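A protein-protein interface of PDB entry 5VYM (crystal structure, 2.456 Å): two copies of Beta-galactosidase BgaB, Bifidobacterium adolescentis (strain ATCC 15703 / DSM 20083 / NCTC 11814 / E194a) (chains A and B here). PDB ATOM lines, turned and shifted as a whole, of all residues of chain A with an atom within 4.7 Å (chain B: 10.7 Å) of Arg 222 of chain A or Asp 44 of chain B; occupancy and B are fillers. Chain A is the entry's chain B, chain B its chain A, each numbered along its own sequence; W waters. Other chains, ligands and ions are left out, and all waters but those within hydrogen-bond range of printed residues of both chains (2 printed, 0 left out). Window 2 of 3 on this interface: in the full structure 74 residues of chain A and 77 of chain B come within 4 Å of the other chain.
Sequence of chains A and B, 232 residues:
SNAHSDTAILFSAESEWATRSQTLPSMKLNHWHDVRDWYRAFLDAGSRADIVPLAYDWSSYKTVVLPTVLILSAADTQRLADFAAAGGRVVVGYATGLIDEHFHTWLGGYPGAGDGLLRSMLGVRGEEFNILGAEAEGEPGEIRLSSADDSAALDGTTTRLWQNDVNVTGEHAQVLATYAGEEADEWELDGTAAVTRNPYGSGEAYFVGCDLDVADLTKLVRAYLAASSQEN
The backbone carbonyl oxygen (O) of Tyr 224 of chain A sits at hydrogen-bond distance from the guanidinium group (NH1) of Arg 89 of chain B, at 3.0 Å. NH2 of Arg 222 of chain A sits at hydrogen-bond distance from O of Asp 44 of chain B.
The backbone carbonyl oxygen of Phe 42 of chain B is in hydrogen-bond range of the backbone NH of Arg 48 of chain B. The side-chain carboxylate (OD1) of Asp 37 of chain B lies within salt-bridge range of the guanidinium group (NH2) of Arg 40 of chain B (3.0 Å). The backbone NH (N) of Ala 226 of chain A sits at hydrogen-bond distance from the backbone carbonyl oxygen (O) of Val 221 of chain A, at 2.8 Å. O of Val 214 of chain A is in hydrogen-bond range of OG1 of Thr 218 of chain A (2.4 Å). The backbone carbonyl oxygen (O) of Phe 42 of chain B lies within hydrogen-bond range of the backbone NH (N) of Ser 47 of chain B (3.1 Å).
Among the printed residues, merely in contact across the chains: Val 214 of chain A with Asp 37 of chain B (3.5 Å), Val 214 of chain A with Arg 40 of chain B (3.8 Å), Thr 218 of chain A with Ala 41 of chain B (3.6 Å), Thr 218 of chain A with Asp 44 of chain B (3.9 Å), Thr 218 of chain A with Ala 45 of chain B (3.8 Å), Val 221 of chain A with Trp 38 of chain B (3.9 Å), Val 221 of chain A with Phe 42 of chain B (3.6 Å), Val 221 of chain A with Ala 45 of chain B (3.7 Å), Arg 222 of chain A with Ala 45 of chain B (3.6 Å) and Ala 226 of chain A with Ser 47 of chain B (3.6 Å).
Printed residues of chain B within 4 Å of Thr 218 of chain A: Ala 41 (3.6 Å), Asp 44 (3.9 Å) and Ala 45 (3.8 Å). Of the printed residues of chain B, Val 221 of chain A touches Trp 38, Phe 42 and Ala 45. Arg 222 of chain A touches just these residues of chain B: Asp 44 (2.9 Å) and Ala 45 (3.6 Å). No residue of chain B comes within 4 Å of Ala 223 of chain A. Arg 36 of chain B touches none of the printed residues of chain A. Of the printed residues of chain A, Arg 40 of chain B touches Val 214 (3.8 Å). Asp 44 of chain B touches two residues of chain A. Of the printed residues of chain A, Ser 47 of chain B touches Ala 226 (3.6 Å). Arg 48 of chain B touches none of the printed residues of chain A. Of the printed residues of chain A, Arg 89 of chain B touches Tyr 224 (3.0 Å). The nearest residue of chain B that does not touch Arg 222 of chain A is Gly 46 of chain B (5.2 Å). The nearest residue of chain A that does not touch Asp 44 of chain B is Val 214 of chain A (4.2 Å).
Hydrophobic or aromatic side chains of chain B that line the printed part of chain A: Trp 38, Ala 41, Phe 42 and Ala 45. Of the 9 printed residues of chain A, 6 touch a printed residue of chain B. Among the printed residues, no Asp or Glu carboxylate lies within 4 Å of a Lys or Arg side-chain nitrogen of the other chain.
No position is printed for both chains.
Water W2 lies within hydrogen-bond range of the side-chain carboxylate of Asp 44 of chain B (2.6 Å) and the side-chain hydroxyl of Thr 218 of chain A (2.7 Å). Water W1 bridges O of Ala 226 of chain A (2.7 Å) and NH1 of Arg 89 of chain B (3.1 Å).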
ATOM      1  N   VAL A 214     -15.452  -1.625 -19.568  1.00  0.00           N
ATOM      2  CA  VAL A 214     -14.271  -0.894 -20.024  1.00  0.00           C
ATOM      3  C   VAL A 214     -13.742   0.022 -18.927  1.00  0.00           C
ATOM      4  O   VAL A 214     -12.525   0.172 -18.759  1.00  0.00           O
ATOM      5  CB  VAL A 214     -14.594  -0.113 -21.311  1.00  0.00           C
ATOM      6  CG1 VAL A 214     -13.379   0.683 -21.772  1.00  0.00           C
ATOM      7  CG2 VAL A 214     -15.063  -1.066 -22.401  1.00  0.00           C
ATOM      8  N   THR A 218     -10.167  -0.664 -17.480  1.00  0.00           N
ATOM      9  CA  THR A 218      -9.110   0.335 -17.598  1.00  0.00           C
ATOM     10  C   THR A 218      -8.355   0.488 -16.283  1.00  0.00           C
ATOM     11  O   THR A 218      -7.133   0.679 -16.281  1.00  0.00           O
ATOM     12  CB  THR A 218      -9.697   1.677 -18.038  1.00  0.00           C
ATOM     13  OG1 THR A 218     -10.520   1.486 -19.195  1.00  0.00           O
ATOM     14  CG2 THR A 218      -8.587   2.659 -18.379  1.00  0.00           C
ATOM     15  N   LYS A 219      -9.068   0.406 -15.155  1.00  0.00           N
ATOM     16  CA  LYS A 219      -8.411   0.424 -13.851  1.00  0.00           C
ATOM     17  C   LYS A 219      -7.402  -0.711 -13.732  1.00  0.00           C
ATOM     18  O   LYS A 219      -6.270  -0.508 -13.278  1.00  0.00           O
ATOM     19  CB  LYS A 219      -9.451   0.323 -12.735  1.00  0.00           C
ATOM     20  CG  LYS A 219     -10.189   1.610 -12.417  1.00  0.00           C
ATOM     21  CD  LYS A 219     -11.037   1.427 -11.167  1.00  0.00           C
ATOM     22  CE  LYS A 219     -11.573   2.747 -10.644  1.00  0.00           C
ATOM     23  NZ  LYS A 219     -12.213   2.580  -9.308  1.00  0.00           N
ATOM     24  N   LEU A 220      -7.803  -1.919 -14.135  1.00  0.00           N
ATOM     25  CA  LEU A 220      -6.912  -3.072 -14.058  1.00  0.00           C
ATOM     26  C   LEU A 220      -5.676  -2.868 -14.927  1.00  0.00           C
ATOM     27  O   LEU A 220      -4.549  -3.135 -14.494  1.00  0.00           O
ATOM     28  CB  LEU A 220      -7.670  -4.334 -14.476  1.00  0.00           C
ATOM     29  CG  LEU A 220      -7.062  -5.718 -14.227  1.00  0.00           C
ATOM     30  CD1 LEU A 220      -8.173  -6.754 -14.162  1.00  0.00           C
ATOM     31  CD2 LEU A 220      -6.052  -6.102 -15.302  1.00  0.00           C
ATOM     32  N   VAL A 221      -5.872  -2.399 -16.160  1.00  0.00           N
ATOM     33  CA  VAL A 221      -4.751  -2.228 -17.080  1.00  0.00           C
ATOM     34  C   VAL A 221      -3.779  -1.184 -16.545  1.00  0.00           C
ATOM     35  O   VAL A 221      -2.560  -1.394 -16.528  1.00  0.00           O
ATOM     36  CB  VAL A 221      -5.259  -1.856 -18.484  1.00  0.00           C
ATOM     37  CG1 VAL A 221      -4.095  -1.485 -19.386  1.00  0.00           C
ATOM     38  CG2 VAL A 221      -6.052  -3.007 -19.082  1.00  0.00           C
ATOM     39  N   ARG A 222      -4.309  -0.048 -16.089  1.00  0.00           N
ATOM     40  CA  ARG A 222      -3.448   1.040 -15.635  1.00  0.00           C
ATOM     41  C   ARG A 222      -2.671   0.657 -14.382  1.00  0.00           C
ATOM     42  O   ARG A 222      -1.539   1.113 -14.190  1.00  0.00           O
ATOM     43  CB  ARG A 222      -4.290   2.293 -15.391  1.00  0.00           C
ATOM     44  CG  ARG A 222      -3.492   3.567 -15.191  1.00  0.00           C
ATOM     45  CD  ARG A 222      -4.425   4.764 -15.150  1.00  0.00           C
ATOM     46  NE  ARG A 222      -5.048   5.014 -16.447  1.00  0.00           N
ATOM     47  CZ  ARG A 222      -6.223   5.613 -16.608  1.00  0.00           C
ATOM     48  NH1 ARG A 222      -6.915   6.012 -15.551  1.00  0.00           N
ATOM     49  NH2 ARG A 222      -6.712   5.804 -17.827  1.00  0.00           N
ATOM     50  N   ALA A 223      -3.251  -0.192 -13.531  1.00  0.00           N
ATOM     51  CA  ALA A 223      -2.586  -0.582 -12.292  1.00  0.00           C
ATOM     52  C   ALA A 223      -1.480  -1.607 -12.530  1.00  0.00           C
ATOM     53  O   ALA A 223      -0.436  -1.556 -11.869  1.00  0.00           O
ATOM     54  CB  ALA A 223      -3.610  -1.134 -11.298  1.00  0.00           C
ATOM     55  N   TYR A 224      -1.681  -2.538 -13.460  1.00  0.00           N
ATOM     56  CA  TYR A 224      -0.779  -3.674 -13.601  1.00  0.00           C
ATOM     57  C   TYR A 224      -0.189  -3.853 -14.993  1.00  0.00           C
ATOM     58  O   TYR A 224       0.930  -4.359 -15.104  1.00  0.00           O
ATOM     59  CB  TYR A 224      -1.498  -4.976 -13.209  1.00  0.00           C
ATOM     60  CG  TYR A 224      -2.060  -4.972 -11.803  1.00  0.00           C
ATOM     61  CD1 TYR A 224      -1.223  -5.087 -10.702  1.00  0.00           C
ATOM     62  CD2 TYR A 224      -3.427  -4.870 -11.579  1.00  0.00           C
ATOM     63  CE1 TYR A 224      -1.729  -5.089  -9.417  1.00  0.00           C
ATOM     64  CE2 TYR A 224      -3.943  -4.873 -10.297  1.00  0.00           C
ATOM     65  CZ  TYR A 224      -3.090  -4.983  -9.221  1.00  0.00           C
ATOM     66  OH  TYR A 224      -3.598  -4.986  -7.942  1.00  0.00           O
ATOM     67  N   ALA A 226       0.024  -1.424 -17.690  1.00  0.00           N
ATOM     68  CA  ALA A 226       0.317  -0.221 -18.452  1.00  0.00           C
ATOM     69  C   ALA A 226       1.821   0.039 -18.474  1.00  0.00           C
ATOM     70  O   ALA A 226       2.619  -0.692 -17.882  1.00  0.00           O
ATOM     71  CB  ALA A 226      -0.442   0.975 -17.877  1.00  0.00           C
ATOM     72  N   THR B   7       1.934  -4.436 -26.330  1.00  0.00           N
ATOM     73  CA  THR B   7       0.879  -5.357 -25.935  1.00  0.00           C
ATOM     74  C   THR B   7       0.106  -5.806 -27.165  1.00  0.00           C
ATOM     75  O   THR B   7      -0.292  -4.978 -27.991  1.00  0.00           O
ATOM     76  CB  THR B   7      -0.071  -4.702 -24.929  1.00  0.00           C
ATOM     77  OG1 THR B   7       0.671  -4.273 -23.780  1.00  0.00           O
ATOM     78  CG2 THR B   7      -1.148  -5.682 -24.494  1.00  0.00           C
ATOM     79  N   ILE B   9      -3.294  -8.043 -28.289  1.00  0.00           N
ATOM     80  CA  ILE B   9      -4.532  -8.718 -27.927  1.00  0.00           C
ATOM     81  C   ILE B   9      -4.809  -9.749 -29.011  1.00  0.00           C
ATOM     82  O   ILE B   9      -5.064  -9.397 -30.168  1.00  0.00           O
ATOM     83  CB  ILE B   9      -5.695  -7.731 -27.773  1.00  0.00           C
ATOM     84  CG1 ILE B   9      -5.333  -6.652 -26.752  1.00  0.00           C
ATOM     85  CG2 ILE B   9      -6.956  -8.462 -27.344  1.00  0.00           C
ATOM     86  CD1 ILE B   9      -6.400  -5.611 -26.576  1.00  0.00           C
ATOM     87  N   ARG B  36     -12.557  -6.368 -28.152  1.00  0.00           N
ATOM     88  CA  ARG B  36     -12.829  -4.952 -28.366  1.00  0.00           C
ATOM     89  C   ARG B  36     -12.776  -4.175 -27.056  1.00  0.00           C
ATOM     90  O   ARG B  36     -12.265  -3.049 -27.014  1.00  0.00           O
ATOM     91  CB  ARG B  36     -14.190  -4.795 -29.042  1.00  0.00           C
ATOM     92  CG  ARG B  36     -14.449  -3.436 -29.649  1.00  0.00           C
ATOM     93  CD  ARG B  36     -15.725  -3.467 -30.471  1.00  0.00           C
ATOM     94  NE  ARG B  36     -16.893  -3.753 -29.643  1.00  0.00           N
ATOM     95  CZ  ARG B  36     -18.037  -4.241 -30.109  1.00  0.00           C
ATOM     96  NH1 ARG B  36     -18.168  -4.513 -31.401  1.00  0.00           N
ATOM     97  NH2 ARG B  36     -19.048  -4.467 -29.282  1.00  0.00           N
ATOM     98  N   ASP B  37     -13.294  -4.759 -25.973  1.00  0.00           N
ATOM     99  CA  ASP B  37     -13.267  -4.072 -24.685  1.00  0.00           C
ATOM    100  C   ASP B  37     -11.849  -3.984 -24.134  1.00  0.00           C
ATOM    101  O   ASP B  37     -11.450  -2.941 -23.600  1.00  0.00           O
ATOM    102  CB  ASP B  37     -14.190  -4.774 -23.690  1.00  0.00           C
ATOM    103  CG  ASP B  37     -15.657  -4.537 -23.993  1.00  0.00           C
ATOM    104  OD1 ASP B  37     -15.967  -3.573 -24.726  1.00  0.00           O
ATOM    105  OD2 ASP B  37     -16.502  -5.309 -23.492  1.00  0.00           O
ATOM    106  N   TRP B  38     -11.071  -5.064 -24.251  1.00  0.00           N
ATOM    107  CA  TRP B  38      -9.673  -5.004 -23.841  1.00  0.00           C
ATOM    108  C   TRP B  38      -8.895  -3.980 -24.655  1.00  0.00           C
ATOM    109  O   TRP B  38      -7.976  -3.339 -24.131  1.00  0.00           O
ATOM    110  CB  TRP B  38      -9.021  -6.382 -23.967  1.00  0.00           C
ATOM    111  CG  TRP B  38      -9.178  -7.250 -22.752  1.00  0.00           C
ATOM    112  CD1 TRP B  38     -10.126  -8.209 -22.546  1.00  0.00           C
ATOM    113  CD2 TRP B  38      -8.356  -7.241 -21.577  1.00  0.00           C
ATOM    114  NE1 TRP B  38      -9.945  -8.800 -21.317  1.00  0.00           N
ATOM    115  CE2 TRP B  38      -8.865  -8.222 -20.702  1.00  0.00           C
ATOM    116  CE3 TRP B  38      -7.239  -6.499 -21.180  1.00  0.00           C
ATOM    117  CZ2 TRP B  38      -8.296  -8.479 -19.455  1.00  0.00           C
ATOM    118  CZ3 TRP B  38      -6.676  -6.756 -19.942  1.00  0.00           C
ATOM    119  CH2 TRP B  38      -7.205  -7.737 -19.094  1.00  0.00           C
ATOM    120  N   TYR B  39      -9.244  -3.810 -25.932  1.00  0.00           N
ATOM    121  CA  TYR B  39      -8.590  -2.793 -26.749  1.00  0.00           C
ATOM    122  C   TYR B  39      -8.927  -1.395 -26.248  1.00  0.00           C
ATOM    123  O   TYR B  39      -8.043  -0.540 -26.117  1.00  0.00           O
ATOM    124  CB  TYR B  39      -8.996  -2.954 -28.214  1.00  0.00           C
ATOM    125  CG  TYR B  39      -8.363  -1.935 -29.135  1.00  0.00           C
ATOM    126  CD1 TYR B  39      -9.013  -0.745 -29.442  1.00  0.00           C
ATOM    127  CD2 TYR B  39      -7.113  -2.160 -29.694  1.00  0.00           C
ATOM    128  CE1 TYR B  39      -8.435   0.191 -30.280  1.00  0.00           C
ATOM    129  CE2 TYR B  39      -6.527  -1.231 -30.535  1.00  0.00           C
ATOM    130  CZ  TYR B  39      -7.192  -0.058 -30.824  1.00  0.00           C
ATOM    131  OH  TYR B  39      -6.611   0.869 -31.659  1.00  0.00           O
ATOM    132  N   ARG B  40     -10.208  -1.143 -25.969  1.00  0.00           N
ATOM    133  CA  ARG B  40     -10.611   0.149 -25.426  1.00  0.00           C
ATOM    134  C   ARG B  40      -9.943   0.415 -24.084  1.00  0.00           C
ATOM    135  O   ARG B  40      -9.561   1.552 -23.786  1.00  0.00           O
ATOM    136  CB  ARG B  40     -12.132   0.206 -25.285  1.00  0.00           C
ATOM    137  CG  ARG B  40     -12.890   0.114 -26.596  1.00  0.00           C
ATOM    138  CD  ARG B  40     -14.323  -0.323 -26.359  1.00  0.00           C
ATOM    139  NE  ARG B  40     -15.110  -0.326 -27.588  1.00  0.00           N
ATOM    140  CZ  ARG B  40     -16.325  -0.854 -27.692  1.00  0.00           C
ATOM    141  NH1 ARG B  40     -16.972  -0.811 -28.847  1.00  0.00           N
ATOM    142  NH2 ARG B  40     -16.890  -1.430 -26.642  1.00  0.00           N
ATOM    143  N   ALA B  41      -9.792  -0.627 -23.261  1.00  0.00           N
ATOM    144  CA  ALA B  41      -9.169  -0.461 -21.953  1.00  0.00           C
ATOM    145  C   ALA B  41      -7.713  -0.030 -22.089  1.00  0.00           C
ATOM    146  O   ALA B  41      -7.266   0.908 -21.419  1.00  0.00           O
ATOM    147  CB  ALA B  41      -9.278  -1.760 -21.153  1.00  0.00           C
ATOM    148  N   PHE B  42      -6.956  -0.707 -22.955  1.00  0.00           N
ATOM    149  CA  PHE B  42      -5.562  -0.328 -23.168  1.00  0.00           C
ATOM    150  C   PHE B  42      -5.443   1.046 -23.816  1.00  0.00           C
ATOM    151  O   PHE B  42      -4.475   1.769 -23.557  1.00  0.00           O
ATOM    152  CB  PHE B  42      -4.853  -1.381 -24.021  1.00  0.00           C
ATOM    153  CG  PHE B  42      -4.286  -2.522 -23.226  1.00  0.00           C
ATOM    154  CD1 PHE B  42      -3.025  -2.428 -22.662  1.00  0.00           C
ATOM    155  CD2 PHE B  42      -5.008  -3.689 -23.048  1.00  0.00           C
ATOM    156  CE1 PHE B  42      -2.497  -3.475 -21.932  1.00  0.00           C
ATOM    157  CE2 PHE B  42      -4.486  -4.739 -22.319  1.00  0.00           C
ATOM    158  CZ  PHE B  42      -3.228  -4.631 -21.760  1.00  0.00           C
ATOM    159  N   LEU B  43      -6.409   1.422 -24.654  1.00  0.00           N
ATOM    160  CA  LEU B  43      -6.366   2.736 -25.287  1.00  0.00           C
ATOM    161  C   LEU B  43      -6.581   3.842 -24.260  1.00  0.00           C
ATOM    162  O   LEU B  43      -5.807   4.806 -24.200  1.00  0.00           O
ATOM    163  CB  LEU B  43      -7.414   2.814 -26.399  1.00  0.00           C
ATOM    164  CG  LEU B  43      -7.444   4.093 -27.238  1.00  0.00           C
ATOM    165  CD1 LEU B  43      -6.106   4.313 -27.924  1.00  0.00           C
ATOM    166  CD2 LEU B  43      -8.571   4.040 -28.258  1.00  0.00           C
ATOM    167  N   ASP B  44      -7.622   3.713 -23.434  1.00  0.00           N
ATOM    168  CA  ASP B  44      -7.902   4.728 -22.423  1.00  0.00           C
ATOM    169  C   ASP B  44      -6.826   4.767 -21.346  1.00  0.00           C
ATOM    170  O   ASP B  44      -6.622   5.811 -20.716  1.00  0.00           O
ATOM    171  CB  ASP B  44      -9.273   4.480 -21.792  1.00  0.00           C
ATOM    172  CG  ASP B  44     -10.411   4.683 -22.774  1.00  0.00           C
ATOM    173  OD1 ASP B  44     -10.142   5.099 -23.919  1.00  0.00           O
ATOM    174  OD2 ASP B  44     -11.575   4.424 -22.398  1.00  0.00           O
ATOM    175  N   ALA B  45      -6.134   3.653 -21.117  1.00  0.00           N
ATOM    176  CA  ALA B  45      -5.067   3.607 -20.127  1.00  0.00           C
ATOM    177  C   ALA B  45      -3.764   4.217 -20.626  1.00  0.00           C
ATOM    178  O   ALA B  45      -2.798   4.280 -19.860  1.00  0.00           O
ATOM    179  CB  ALA B  45      -4.819   2.164 -19.684  1.00  0.00           C
ATOM    180  N   GLY B  46      -3.711   4.659 -21.882  1.00  0.00           N
ATOM    181  CA  GLY B  46      -2.522   5.268 -22.434  1.00  0.00           C
ATOM    182  C   GLY B  46      -1.535   4.309 -23.065  1.00  0.00           C
ATOM    183  O   GLY B  46      -0.584   4.763 -23.714  1.00  0.00           O
ATOM    184  N   SER B  47      -1.724   3.003 -22.897  1.00  0.00           N
ATOM    185  CA  SER B  47      -0.836   1.997 -23.468  1.00  0.00           C
ATOM    186  C   SER B  47      -1.590   1.222 -24.546  1.00  0.00           C
ATOM    187  O   SER B  47      -1.964   0.060 -24.368  1.00  0.00           O
ATOM    188  CB  SER B  47      -0.304   1.069 -22.369  1.00  0.00           C
ATOM    189  OG  SER B  47       0.552   1.771 -21.484  1.00  0.00           O
ATOM    190  N   ARG B  48      -1.809   1.890 -25.678  1.00  0.00           N
ATOM    191  CA  ARG B  48      -2.572   1.307 -26.775  1.00  0.00           C
ATOM    192  C   ARG B  48      -1.950  -0.005 -27.229  1.00  0.00           C
ATOM    193  O   ARG B  48      -0.734  -0.098 -27.423  1.00  0.00           O
ATOM    194  CB  ARG B  48      -2.644   2.288 -27.945  1.00  0.00           C
ATOM    195  CG  ARG B  48      -3.510   1.812 -29.098  1.00  0.00           C
ATOM    196  CD  ARG B  48      -3.200   2.576 -30.376  1.00  0.00           C
ATOM    197  NE  ARG B  48      -1.813   2.388 -30.788  1.00  0.00           N
ATOM    198  CZ  ARG B  48      -1.369   1.321 -31.447  1.00  0.00           C
ATOM    199  NH1 ARG B  48      -2.206   0.343 -31.770  1.00  0.00           N
ATOM    200  NH2 ARG B  48      -0.089   1.229 -31.784  1.00  0.00           N
ATOM    201  N   ALA B  49      -2.791  -1.018 -27.395  1.00  0.00           N
ATOM    202  CA  ALA B  49      -2.354  -2.345 -27.796  1.00  0.00           C
ATOM    203  C   ALA B  49      -2.710  -2.610 -29.253  1.00  0.00           C
ATOM    204  O   ALA B  49      -3.558  -1.939 -29.846  1.00  0.00           O
ATOM    205  CB  ALA B  49      -2.985  -3.415 -26.903  1.00  0.00           C
ATOM    206  N   ARG B  89       4.847 -11.724 -20.815  1.00  0.00           N
ATOM    207  CA  ARG B  89       3.711 -11.640 -19.909  1.00  0.00           C
ATOM    208  C   ARG B  89       2.448 -12.079 -20.639  1.00  0.00           C
ATOM    209  O   ARG B  89       2.141 -11.566 -21.720  1.00  0.00           O
ATOM    210  CB  ARG B  89       3.551 -10.219 -19.365  1.00  0.00           C
ATOM    211  CG  ARG B  89       2.385 -10.050 -18.402  1.00  0.00           C
ATOM    212  CD  ARG B  89       2.452  -8.710 -17.682  1.00  0.00           C
ATOM    213  NE  ARG B  89       2.446  -7.583 -18.610  1.00  0.00           N
ATOM    214  CZ  ARG B  89       2.565  -6.312 -18.240  1.00  0.00           C
ATOM    215  NH1 ARG B  89       2.702  -6.001 -16.957  1.00  0.00           N
ATOM    216  NH2 ARG B  89       2.550  -5.350 -19.152  1.00  0.00           N
HETATM  217  O   HOH W   1       3.671  -3.071 -17.314  1.00  0.00           O
HETATM  218  O   HOH W   2     -11.862   3.679 -19.924  1.00  0.00           O
